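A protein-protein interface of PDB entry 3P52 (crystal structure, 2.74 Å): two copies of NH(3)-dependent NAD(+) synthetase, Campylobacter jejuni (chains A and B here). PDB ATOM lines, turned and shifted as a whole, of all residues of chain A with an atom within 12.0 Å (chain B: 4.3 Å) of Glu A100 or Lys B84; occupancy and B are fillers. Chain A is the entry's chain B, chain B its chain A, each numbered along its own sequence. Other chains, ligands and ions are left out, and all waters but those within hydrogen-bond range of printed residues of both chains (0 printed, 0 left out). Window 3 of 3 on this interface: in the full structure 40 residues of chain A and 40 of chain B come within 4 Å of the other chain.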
ATOM      1  N   LEU A  92      17.095 -28.886 -17.047  1.00  0.00           N
ATOM      2  CA  LEU A  92      16.675 -27.756 -16.196  1.00  0.00           C
ATOM      3  C   LEU A  92      17.718 -26.668 -16.104  1.00  0.00           C
ATOM      4  O   LEU A  92      17.411 -25.491 -16.266  1.00  0.00           O
ATOM      5  CB  LEU A  92      16.285 -28.219 -14.824  1.00  0.00           C
ATOM      6  CG  LEU A  92      15.582 -27.233 -13.911  1.00  0.00           C
ATOM      7  CD1 LEU A  92      14.388 -26.588 -14.629  1.00  0.00           C
ATOM      8  CD2 LEU A  92      15.157 -28.033 -12.645  1.00  0.00           C
ATOM      9  N   ASP A  93      18.966 -27.026 -15.898  1.00  0.00           N
ATOM     10  CA  ASP A  93      19.989 -25.996 -15.914  1.00  0.00           C
ATOM     11  C   ASP A  93      19.998 -25.247 -17.238  1.00  0.00           C
ATOM     12  O   ASP A  93      20.329 -24.045 -17.284  1.00  0.00           O
ATOM     13  CB  ASP A  93      21.382 -26.574 -15.731  1.00  0.00           C
ATOM     14  CG  ASP A  93      21.643 -27.138 -14.331  1.00  0.00           C
ATOM     15  OD1 ASP A  93      20.915 -26.849 -13.345  1.00  0.00           O
ATOM     16  OD2 ASP A  93      22.650 -27.871 -14.237  1.00  0.00           O
ATOM     17  N   ALA A  94      19.653 -25.947 -18.335  1.00  0.00           N
ATOM     18  CA  ALA A  94      19.825 -25.316 -19.638  1.00  0.00           C
ATOM     19  C   ALA A  94      18.753 -24.246 -19.828  1.00  0.00           C
ATOM     20  O   ALA A  94      19.042 -23.159 -20.352  1.00  0.00           O
ATOM     21  CB  ALA A  94      19.798 -26.330 -20.728  1.00  0.00           C
ATOM     22  N   PHE A  95      17.540 -24.533 -19.366  1.00  0.00           N
ATOM     23  CA  PHE A  95      16.495 -23.512 -19.359  1.00  0.00           C
ATOM     24  C   PHE A  95      16.845 -22.281 -18.472  1.00  0.00           C
ATOM     25  O   PHE A  95      16.708 -21.161 -18.877  1.00  0.00           O
ATOM     26  CB  PHE A  95      15.188 -24.107 -18.885  1.00  0.00           C
ATOM     27  CG  PHE A  95      14.440 -24.795 -19.936  1.00  0.00           C
ATOM     28  CD1 PHE A  95      13.858 -24.084 -20.973  1.00  0.00           C
ATOM     29  CD2 PHE A  95      14.289 -26.165 -19.886  1.00  0.00           C
ATOM     30  CE1 PHE A  95      13.136 -24.713 -21.930  1.00  0.00           C
ATOM     31  CE2 PHE A  95      13.549 -26.830 -20.876  1.00  0.00           C
ATOM     32  CZ  PHE A  95      12.972 -26.094 -21.892  1.00  0.00           C
ATOM     33  N   ILE A  96      17.334 -22.541 -17.268  1.00  0.00           N
ATOM     34  CA  ILE A  96      17.418 -21.546 -16.239  1.00  0.00           C
ATOM     35  C   ILE A  96      18.386 -20.532 -16.782  1.00  0.00           C
ATOM     36  O   ILE A  96      18.242 -19.322 -16.582  1.00  0.00           O
ATOM     37  CB  ILE A  96      17.878 -22.226 -14.926  1.00  0.00           C
ATOM     38  CG1 ILE A  96      16.657 -22.733 -14.167  1.00  0.00           C
ATOM     39  CG2 ILE A  96      18.709 -21.319 -14.064  1.00  0.00           C
ATOM     40  CD1 ILE A  96      17.027 -23.678 -13.080  1.00  0.00           C
ATOM     41  N   LYS A  97      19.342 -21.023 -17.545  1.00  0.00           N
ATOM     42  CA  LYS A  97      20.379 -20.174 -18.104  1.00  0.00           C
ATOM     43  C   LYS A  97      19.794 -19.200 -19.114  1.00  0.00           C
ATOM     44  O   LYS A  97      20.399 -18.191 -19.455  1.00  0.00           O
ATOM     45  CB  LYS A  97      21.408 -21.062 -18.764  1.00  0.00           C
ATOM     46  CG  LYS A  97      22.626 -20.403 -19.246  1.00  0.00           C
ATOM     47  CD  LYS A  97      23.757 -21.436 -19.259  1.00  0.00           C
ATOM     48  CE  LYS A  97      24.623 -21.324 -20.539  1.00  0.00           C
ATOM     49  NZ  LYS A  97      25.419 -20.059 -20.516  1.00  0.00           N
ATOM     50  N   GLN A  98      18.600 -19.481 -19.599  1.00  0.00           N
ATOM     51  CA  GLN A  98      18.020 -18.593 -20.571  1.00  0.00           C
ATOM     52  C   GLN A  98      16.891 -17.778 -19.966  1.00  0.00           C
ATOM     53  O   GLN A  98      16.210 -17.013 -20.690  1.00  0.00           O
ATOM     54  CB  GLN A  98      17.498 -19.393 -21.751  1.00  0.00           C
ATOM     55  CG  GLN A  98      18.477 -20.309 -22.414  1.00  0.00           C
ATOM     56  CD  GLN A  98      19.711 -19.602 -22.806  1.00  0.00           C
ATOM     57  OE1 GLN A  98      19.675 -18.426 -23.083  1.00  0.00           O
ATOM     58  NE2 GLN A  98      20.846 -20.296 -22.776  1.00  0.00           N
ATOM     59  N   SER A  99      16.680 -17.962 -18.656  1.00  0.00           N
ATOM     60  CA  SER A  99      15.573 -17.339 -17.932  1.00  0.00           C
ATOM     61  C   SER A  99      16.045 -16.060 -17.226  1.00  0.00           C
ATOM     62  O   SER A  99      17.201 -15.925 -16.874  1.00  0.00           O
ATOM     63  CB  SER A  99      14.945 -18.309 -16.940  1.00  0.00           C
ATOM     64  OG  SER A  99      14.028 -17.625 -16.104  1.00  0.00           O
ATOM     65  N   GLU A 100      15.145 -15.122 -17.061  1.00  0.00           N
ATOM     66  CA  GLU A 100      15.503 -13.888 -16.444  1.00  0.00           C
ATOM     67  C   GLU A 100      14.788 -13.795 -15.138  1.00  0.00           C
ATOM     68  O   GLU A 100      14.922 -12.837 -14.422  1.00  0.00           O
ATOM     69  CB  GLU A 100      15.145 -12.727 -17.345  1.00  0.00           C
ATOM     70  CG  GLU A 100      16.331 -12.169 -18.066  1.00  0.00           C
ATOM     71  CD  GLU A 100      15.971 -11.060 -18.994  1.00  0.00           C
ATOM     72  OE1 GLU A 100      15.177 -10.200 -18.602  1.00  0.00           O
ATOM     73  OE2 GLU A 100      16.481 -11.036 -20.121  1.00  0.00           O
ATOM     74  N   ASN A 101      14.045 -14.823 -14.795  1.00  0.00           N
ATOM     75  CA  ASN A 101      13.361 -14.769 -13.534  1.00  0.00           C
ATOM     76  C   ASN A 101      13.512 -15.967 -12.639  1.00  0.00           C
ATOM     77  O   ASN A 101      12.702 -16.846 -12.665  1.00  0.00           O
ATOM     78  CB  ASN A 101      11.887 -14.470 -13.750  1.00  0.00           C
ATOM     79  CG  ASN A 101      11.144 -15.630 -14.235  1.00  0.00           C
ATOM     80  OD1 ASN A 101       9.940 -15.690 -14.134  1.00  0.00           O
ATOM     81  ND2 ASN A 101      11.854 -16.572 -14.783  1.00  0.00           N
ATOM     82  N   THR A 102      14.533 -15.963 -11.806  1.00  0.00           N
ATOM     83  CA  THR A 102      14.744 -17.008 -10.820  1.00  0.00           C
ATOM     84  C   THR A 102      13.649 -17.069  -9.771  1.00  0.00           C
ATOM     85  O   THR A 102      13.499 -16.151  -8.992  1.00  0.00           O
ATOM     86  CB  THR A 102      16.011 -16.720 -10.043  1.00  0.00           C
ATOM     87  OG1 THR A 102      15.751 -15.691  -9.087  1.00  0.00           O
ATOM     88  CG2 THR A 102      17.069 -16.234 -10.969  1.00  0.00           C
ATOM     89  N   THR A 103      12.899 -18.154  -9.716  1.00  0.00           N
ATOM     90  CA  THR A 103      11.905 -18.272  -8.679  1.00  0.00           C
ATOM     91  C   THR A 103      11.366 -19.666  -8.529  1.00  0.00           C
ATOM     92  O   THR A 103      10.932 -20.281  -9.461  1.00  0.00           O
ATOM     93  CB  THR A 103      10.788 -17.259  -8.848  1.00  0.00           C
ATOM     94  OG1 THR A 103       9.721 -17.837  -9.580  1.00  0.00           O
ATOM     95  CG2 THR A 103      11.283 -16.103  -9.601  1.00  0.00           C
ATOM     96  N   LEU A 104      11.404 -20.165  -7.298  1.00  0.00           N
ATOM     97  CA  LEU A 104      10.918 -21.507  -6.999  1.00  0.00           C
ATOM     98  C   LEU A 104       9.755 -21.925  -7.892  1.00  0.00           C
ATOM     99  O   LEU A 104       9.669 -23.076  -8.319  1.00  0.00           O
ATOM    100  CB  LEU A 104      10.453 -21.597  -5.544  1.00  0.00           C
ATOM    101  CG  LEU A 104      11.552 -21.738  -4.489  1.00  0.00           C
ATOM    102  CD1 LEU A 104      12.502 -20.550  -4.540  1.00  0.00           C
ATOM    103  CD2 LEU A 104      10.949 -21.888  -3.101  1.00  0.00           C
ATOM    104  N   VAL A 105       8.861 -20.981  -8.171  1.00  0.00           N
ATOM    105  CA  VAL A 105       7.724 -21.237  -9.048  1.00  0.00           C
ATOM    106  C   VAL A 105       8.169 -21.401 -10.498  1.00  0.00           C
ATOM    107  O   VAL A 105       7.617 -22.216 -11.237  1.00  0.00           O
ATOM    108  CB  VAL A 105       6.683 -20.105  -8.965  1.00  0.00           C
ATOM    109  CG1 VAL A 105       5.546 -20.358  -9.944  1.00  0.00           C
ATOM    110  CG2 VAL A 105       6.153 -19.975  -7.545  1.00  0.00           C
ATOM    111  N   SER A 106       9.169 -20.623 -10.896  1.00  0.00           N
ATOM    112  CA  SER A 106       9.676 -20.677 -12.225  1.00  0.00           C
ATOM    113  C   SER A 106      10.345 -21.992 -12.457  1.00  0.00           C
ATOM    114  O   SER A 106      10.154 -22.594 -13.467  1.00  0.00           O
ATOM    115  CB  SER A 106      10.670 -19.571 -12.377  1.00  0.00           C
ATOM    116  OG  SER A 106      11.057 -19.443 -13.707  1.00  0.00           O
ATOM    117  N   LEU A 107      11.140 -22.445 -11.515  1.00  0.00           N
ATOM    118  CA  LEU A 107      11.750 -23.764 -11.654  1.00  0.00           C
ATOM    119  C   LEU A 107      10.739 -24.890 -11.818  1.00  0.00           C
ATOM    120  O   LEU A 107      10.917 -25.771 -12.672  1.00  0.00           O
ATOM    121  CB  LEU A 107      12.570 -24.104 -10.428  1.00  0.00           C
ATOM    122  CG  LEU A 107      14.069 -23.857 -10.419  1.00  0.00           C
ATOM    123  CD1 LEU A 107      14.425 -22.384 -10.364  1.00  0.00           C
ATOM    124  CD2 LEU A 107      14.654 -24.671  -9.230  1.00  0.00           C
ATOM    125  N   PHE A 110       9.204 -25.142 -15.249  1.00  0.00           N
ATOM    126  CA  PHE A 110      10.110 -25.713 -16.211  1.00  0.00           C
ATOM    127  C   PHE A 110      10.118 -27.207 -15.965  1.00  0.00           C
ATOM    128  O   PHE A 110       9.874 -28.017 -16.889  1.00  0.00           O
ATOM    129  CB  PHE A 110      11.509 -25.224 -16.022  1.00  0.00           C
ATOM    130  CG  PHE A 110      11.820 -23.912 -16.708  1.00  0.00           C
ATOM    131  CD1 PHE A 110      11.488 -23.691 -18.040  1.00  0.00           C
ATOM    132  CD2 PHE A 110      12.523 -22.904 -16.025  1.00  0.00           C
ATOM    133  CE1 PHE A 110      11.804 -22.470 -18.694  1.00  0.00           C
ATOM    134  CE2 PHE A 110      12.842 -21.670 -16.681  1.00  0.00           C
ATOM    135  CZ  PHE A 110      12.479 -21.471 -18.026  1.00  0.00           C
ATOM    136  N   PHE B  55       5.992  -8.060 -26.373  1.00  0.00           N
ATOM    137  CA  PHE B  55       7.352  -8.591 -26.286  1.00  0.00           C
ATOM    138  C   PHE B  55       7.519  -9.843 -27.140  1.00  0.00           C
ATOM    139  O   PHE B  55       6.644 -10.698 -27.183  1.00  0.00           O
ATOM    140  CB  PHE B  55       7.702  -8.881 -24.833  1.00  0.00           C
ATOM    141  CG  PHE B  55       9.103  -9.274 -24.628  1.00  0.00           C
ATOM    142  CD1 PHE B  55      10.105  -8.317 -24.566  1.00  0.00           C
ATOM    143  CD2 PHE B  55       9.449 -10.629 -24.531  1.00  0.00           C
ATOM    144  CE1 PHE B  55      11.410  -8.686 -24.394  1.00  0.00           C
ATOM    145  CE2 PHE B  55      10.776 -11.023 -24.355  1.00  0.00           C
ATOM    146  CZ  PHE B  55      11.753 -10.045 -24.286  1.00  0.00           C
ATOM    147  N   ALA B  56       8.644  -9.957 -27.835  1.00  0.00           N
ATOM    148  CA  ALA B  56       8.837 -11.133 -28.684  1.00  0.00           C
ATOM    149  C   ALA B  56      10.064 -11.920 -28.252  1.00  0.00           C
ATOM    150  O   ALA B  56      11.066 -11.323 -27.824  1.00  0.00           O
ATOM    151  CB  ALA B  56       8.970 -10.709 -30.104  1.00  0.00           C
ATOM    152  N   LEU B  57       9.982 -13.244 -28.311  1.00  0.00           N
ATOM    153  CA  LEU B  57      11.156 -14.079 -28.220  1.00  0.00           C
ATOM    154  C   LEU B  57      11.442 -14.599 -29.605  1.00  0.00           C
ATOM    155  O   LEU B  57      10.517 -15.087 -30.246  1.00  0.00           O
ATOM    156  CB  LEU B  57      10.876 -15.269 -27.336  1.00  0.00           C
ATOM    157  CG  LEU B  57      10.751 -15.062 -25.845  1.00  0.00           C
ATOM    158  CD1 LEU B  57      10.632 -16.405 -25.213  1.00  0.00           C
ATOM    159  CD2 LEU B  57      11.948 -14.386 -25.296  1.00  0.00           C
ATOM    160  N   LEU B  58      12.683 -14.523 -30.035  1.00  0.00           N
ATOM    161  CA  LEU B  58      13.140 -15.122 -31.256  1.00  0.00           C
ATOM    162  C   LEU B  58      14.006 -16.287 -30.875  1.00  0.00           C
ATOM    163  O   LEU B  58      15.032 -16.096 -30.306  1.00  0.00           O
ATOM    164  CB  LEU B  58      13.989 -14.124 -32.014  1.00  0.00           C
ATOM    165  CG  LEU B  58      13.336 -12.969 -32.754  1.00  0.00           C
ATOM    166  CD1 LEU B  58      12.607 -12.069 -31.859  1.00  0.00           C
ATOM    167  CD2 LEU B  58      14.357 -12.215 -33.444  1.00  0.00           C
ATOM    168  N   TYR B  83      12.254  -7.300 -27.721  1.00  0.00           N
ATOM    169  CA  TYR B  83      12.429  -8.695 -28.001  1.00  0.00           C
ATOM    170  C   TYR B  83      13.734  -9.214 -27.374  1.00  0.00           C
ATOM    171  O   TYR B  83      14.511  -8.462 -26.767  1.00  0.00           O
ATOM    172  CB  TYR B  83      12.473  -8.861 -29.506  1.00  0.00           C
ATOM    173  CG  TYR B  83      13.789  -8.371 -30.080  1.00  0.00           C
ATOM    174  CD1 TYR B  83      14.878  -9.249 -30.241  1.00  0.00           C
ATOM    175  CD2 TYR B  83      13.967  -7.026 -30.418  1.00  0.00           C
ATOM    176  CE1 TYR B  83      16.063  -8.804 -30.748  1.00  0.00           C
ATOM    177  CE2 TYR B  83      15.177  -6.580 -30.932  1.00  0.00           C
ATOM    178  CZ  TYR B  83      16.199  -7.482 -31.103  1.00  0.00           C
ATOM    179  OH  TYR B  83      17.384  -7.048 -31.578  1.00  0.00           O
ATOM    180  N   LYS B  84      13.956 -10.511 -27.529  1.00  0.00           N
ATOM    181  CA  LYS B  84      15.200 -11.135 -27.116  1.00  0.00           C
ATOM    182  C   LYS B  84      15.445 -12.381 -27.978  1.00  0.00           C
ATOM    183  O   LYS B  84      14.504 -13.166 -28.277  1.00  0.00           O
ATOM    184  CB  LYS B  84      15.185 -11.463 -25.644  1.00  0.00           C
ATOM    185  CG  LYS B  84      16.482 -11.950 -25.149  1.00  0.00           C
ATOM    186  CD  LYS B  84      16.417 -12.190 -23.656  1.00  0.00           C
ATOM    187  CE  LYS B  84      17.734 -12.766 -23.145  1.00  0.00           C
ATOM    188  NZ  LYS B  84      18.013 -12.377 -21.695  1.00  0.00           N
ATOM    189  N   ILE B  85      16.685 -12.526 -28.437  1.00  0.00           N
ATOM    190  CA  ILE B  85      17.039 -13.651 -29.247  1.00  0.00           C
ATOM    191  C   ILE B  85      17.467 -14.705 -28.252  1.00  0.00           C
ATOM    192  O   ILE B  85      18.227 -14.400 -27.353  1.00  0.00           O
ATOM    193  CB  ILE B  85      18.203 -13.326 -30.163  1.00  0.00           C
ATOM    194  CG1 ILE B  85      17.746 -12.354 -31.250  1.00  0.00           C
ATOM    195  CG2 ILE B  85      18.713 -14.604 -30.805  1.00  0.00           C
ATOM    196  CD1 ILE B  85      18.861 -11.701 -31.942  1.00  0.00           C
ATOM    197  N   ILE B  86      16.945 -15.914 -28.342  1.00  0.00           N
ATOM    198  CA  ILE B  86      17.464 -16.953 -27.486  1.00  0.00           C
ATOM    199  C   ILE B  86      17.697 -18.181 -28.354  1.00  0.00           C
ATOM    200  O   ILE B  86      16.765 -18.688 -28.961  1.00  0.00           O
ATOM    201  CB  ILE B  86      16.508 -17.340 -26.399  1.00  0.00           C
ATOM    202  CG1 ILE B  86      16.188 -16.170 -25.506  1.00  0.00           C
ATOM    203  CG2 ILE B  86      17.110 -18.417 -25.595  1.00  0.00           C
ATOM    204  CD1 ILE B  86      15.060 -16.537 -24.474  1.00  0.00           C
ATOM    205  N   TYR B 122       8.738 -16.273 -19.856  1.00  0.00           N
ATOM    206  CA  TYR B 122       8.775 -14.831 -20.062  1.00  0.00           C
ATOM    207  C   TYR B 122       7.428 -14.191 -19.808  1.00  0.00           C
ATOM    208  O   TYR B 122       7.354 -13.071 -19.273  1.00  0.00           O
ATOM    209  CB  TYR B 122       9.348 -14.457 -21.417  1.00  0.00           C
ATOM    210  CG  TYR B 122      10.879 -14.510 -21.378  1.00  0.00           C
ATOM    211  CD1 TYR B 122      11.636 -13.341 -21.219  1.00  0.00           C
ATOM    212  CD2 TYR B 122      11.580 -15.737 -21.471  1.00  0.00           C
ATOM    213  CE1 TYR B 122      13.029 -13.385 -21.189  1.00  0.00           C
ATOM    214  CE2 TYR B 122      12.980 -15.764 -21.421  1.00  0.00           C
ATOM    215  CZ  TYR B 122      13.674 -14.592 -21.278  1.00  0.00           C
ATOM    216  OH  TYR B 122      15.028 -14.630 -21.226  1.00  0.00           O
ATOM    217  N   LEU B 125       7.384 -13.627 -15.965  1.00  0.00           N
ATOM    218  CA  LEU B 125       8.248 -12.449 -15.874  1.00  0.00           C
ATOM    219  C   LEU B 125       7.517 -11.148 -16.220  1.00  0.00           C
ATOM    220  O   LEU B 125       7.489 -10.234 -15.408  1.00  0.00           O
ATOM    221  CB  LEU B 125       9.487 -12.561 -16.780  1.00  0.00           C
ATOM    222  CG  LEU B 125      10.594 -11.485 -16.620  1.00  0.00           C
ATOM    223  CD1 LEU B 125      11.305 -11.619 -15.274  1.00  0.00           C
ATOM    224  CD2 LEU B 125      11.651 -11.491 -17.720  1.00  0.00           C
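The side-chain hydroxyl (OG) of Ser A99 lies within hydrogen-bond range of the side-chain amide nitrogen (ND2) of Asn A101, 2.8 Å away.
The backbone carbonyl oxygen (O) of Ala B56 is in hydrogen-bond range of the backbone NH (N) of Lys B84 (3.0 Å).
N of Ile B86 sits at hydrogen-bond distance from O of Leu B58 (2.7 Å).
The side-chain hydroxyl (OG) of Ser A106 lies within hydrogen-bond range of the side-chain amide nitrogen (ND2) of Asn A101 (3.2 Å).
The backbone carbonyl oxygen (O) of Lys B84 sits at hydrogen-bond distance from the backbone NH (N) of Leu B58, at 2.9 Å.
Glu A100 touches just these residues of chain B: Lys B84 (2.6 Å) and Leu B125 (3.7 Å).
Of the printed residues of chain B, Asn A101 touches Leu B125 (3.3 Å).
No residue of chain A comes within 4 Å of Ala B56.
No residue of chain A comes within 4 Å of Leu B58.
No residue of chain A comes within 4 Å of Tyr B83.
Of chain A, only Glu A100 comes within 4 Å of Lys B84.
Of chain A, only Gln A98 comes within 4 Å of Ile B86.
Of the printed residues of chain A, Tyr B122 touches Gln A98 (2.7 Å).
Leu B125 touches just these residues of chain A: Glu A100 (3.7 Å) and Asn A101 (3.3 Å).
The nearest printed residue of chain A that does not touch Tyr B122 is Glu A100 (4.03 Å).
No position is printed for both chains.
Among the printed residues, pairs that only touch across the chains: Asn A101 with Leu B125, Gln A98 with Ile B86 and Glu A100 with Leu B125.
Along chain B the printed residues that touch a printed residue of chain A span positions 84 to 125.
Of the 17 printed residues of chain A, 3 touch a printed residue of chain B.
Along chain A the printed residues that touch a printed residue of chain B span positions 98 to 101.
The backbone carbonyl oxygen (O) of Gln A98 is in hydrogen-bond range of the side-chain hydroxyl (OH) of Tyr B122, 2.7 Å away.
OE2 of Glu A100 is in salt-bridge range of NZ of Lys B84, 2.6 Å away.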
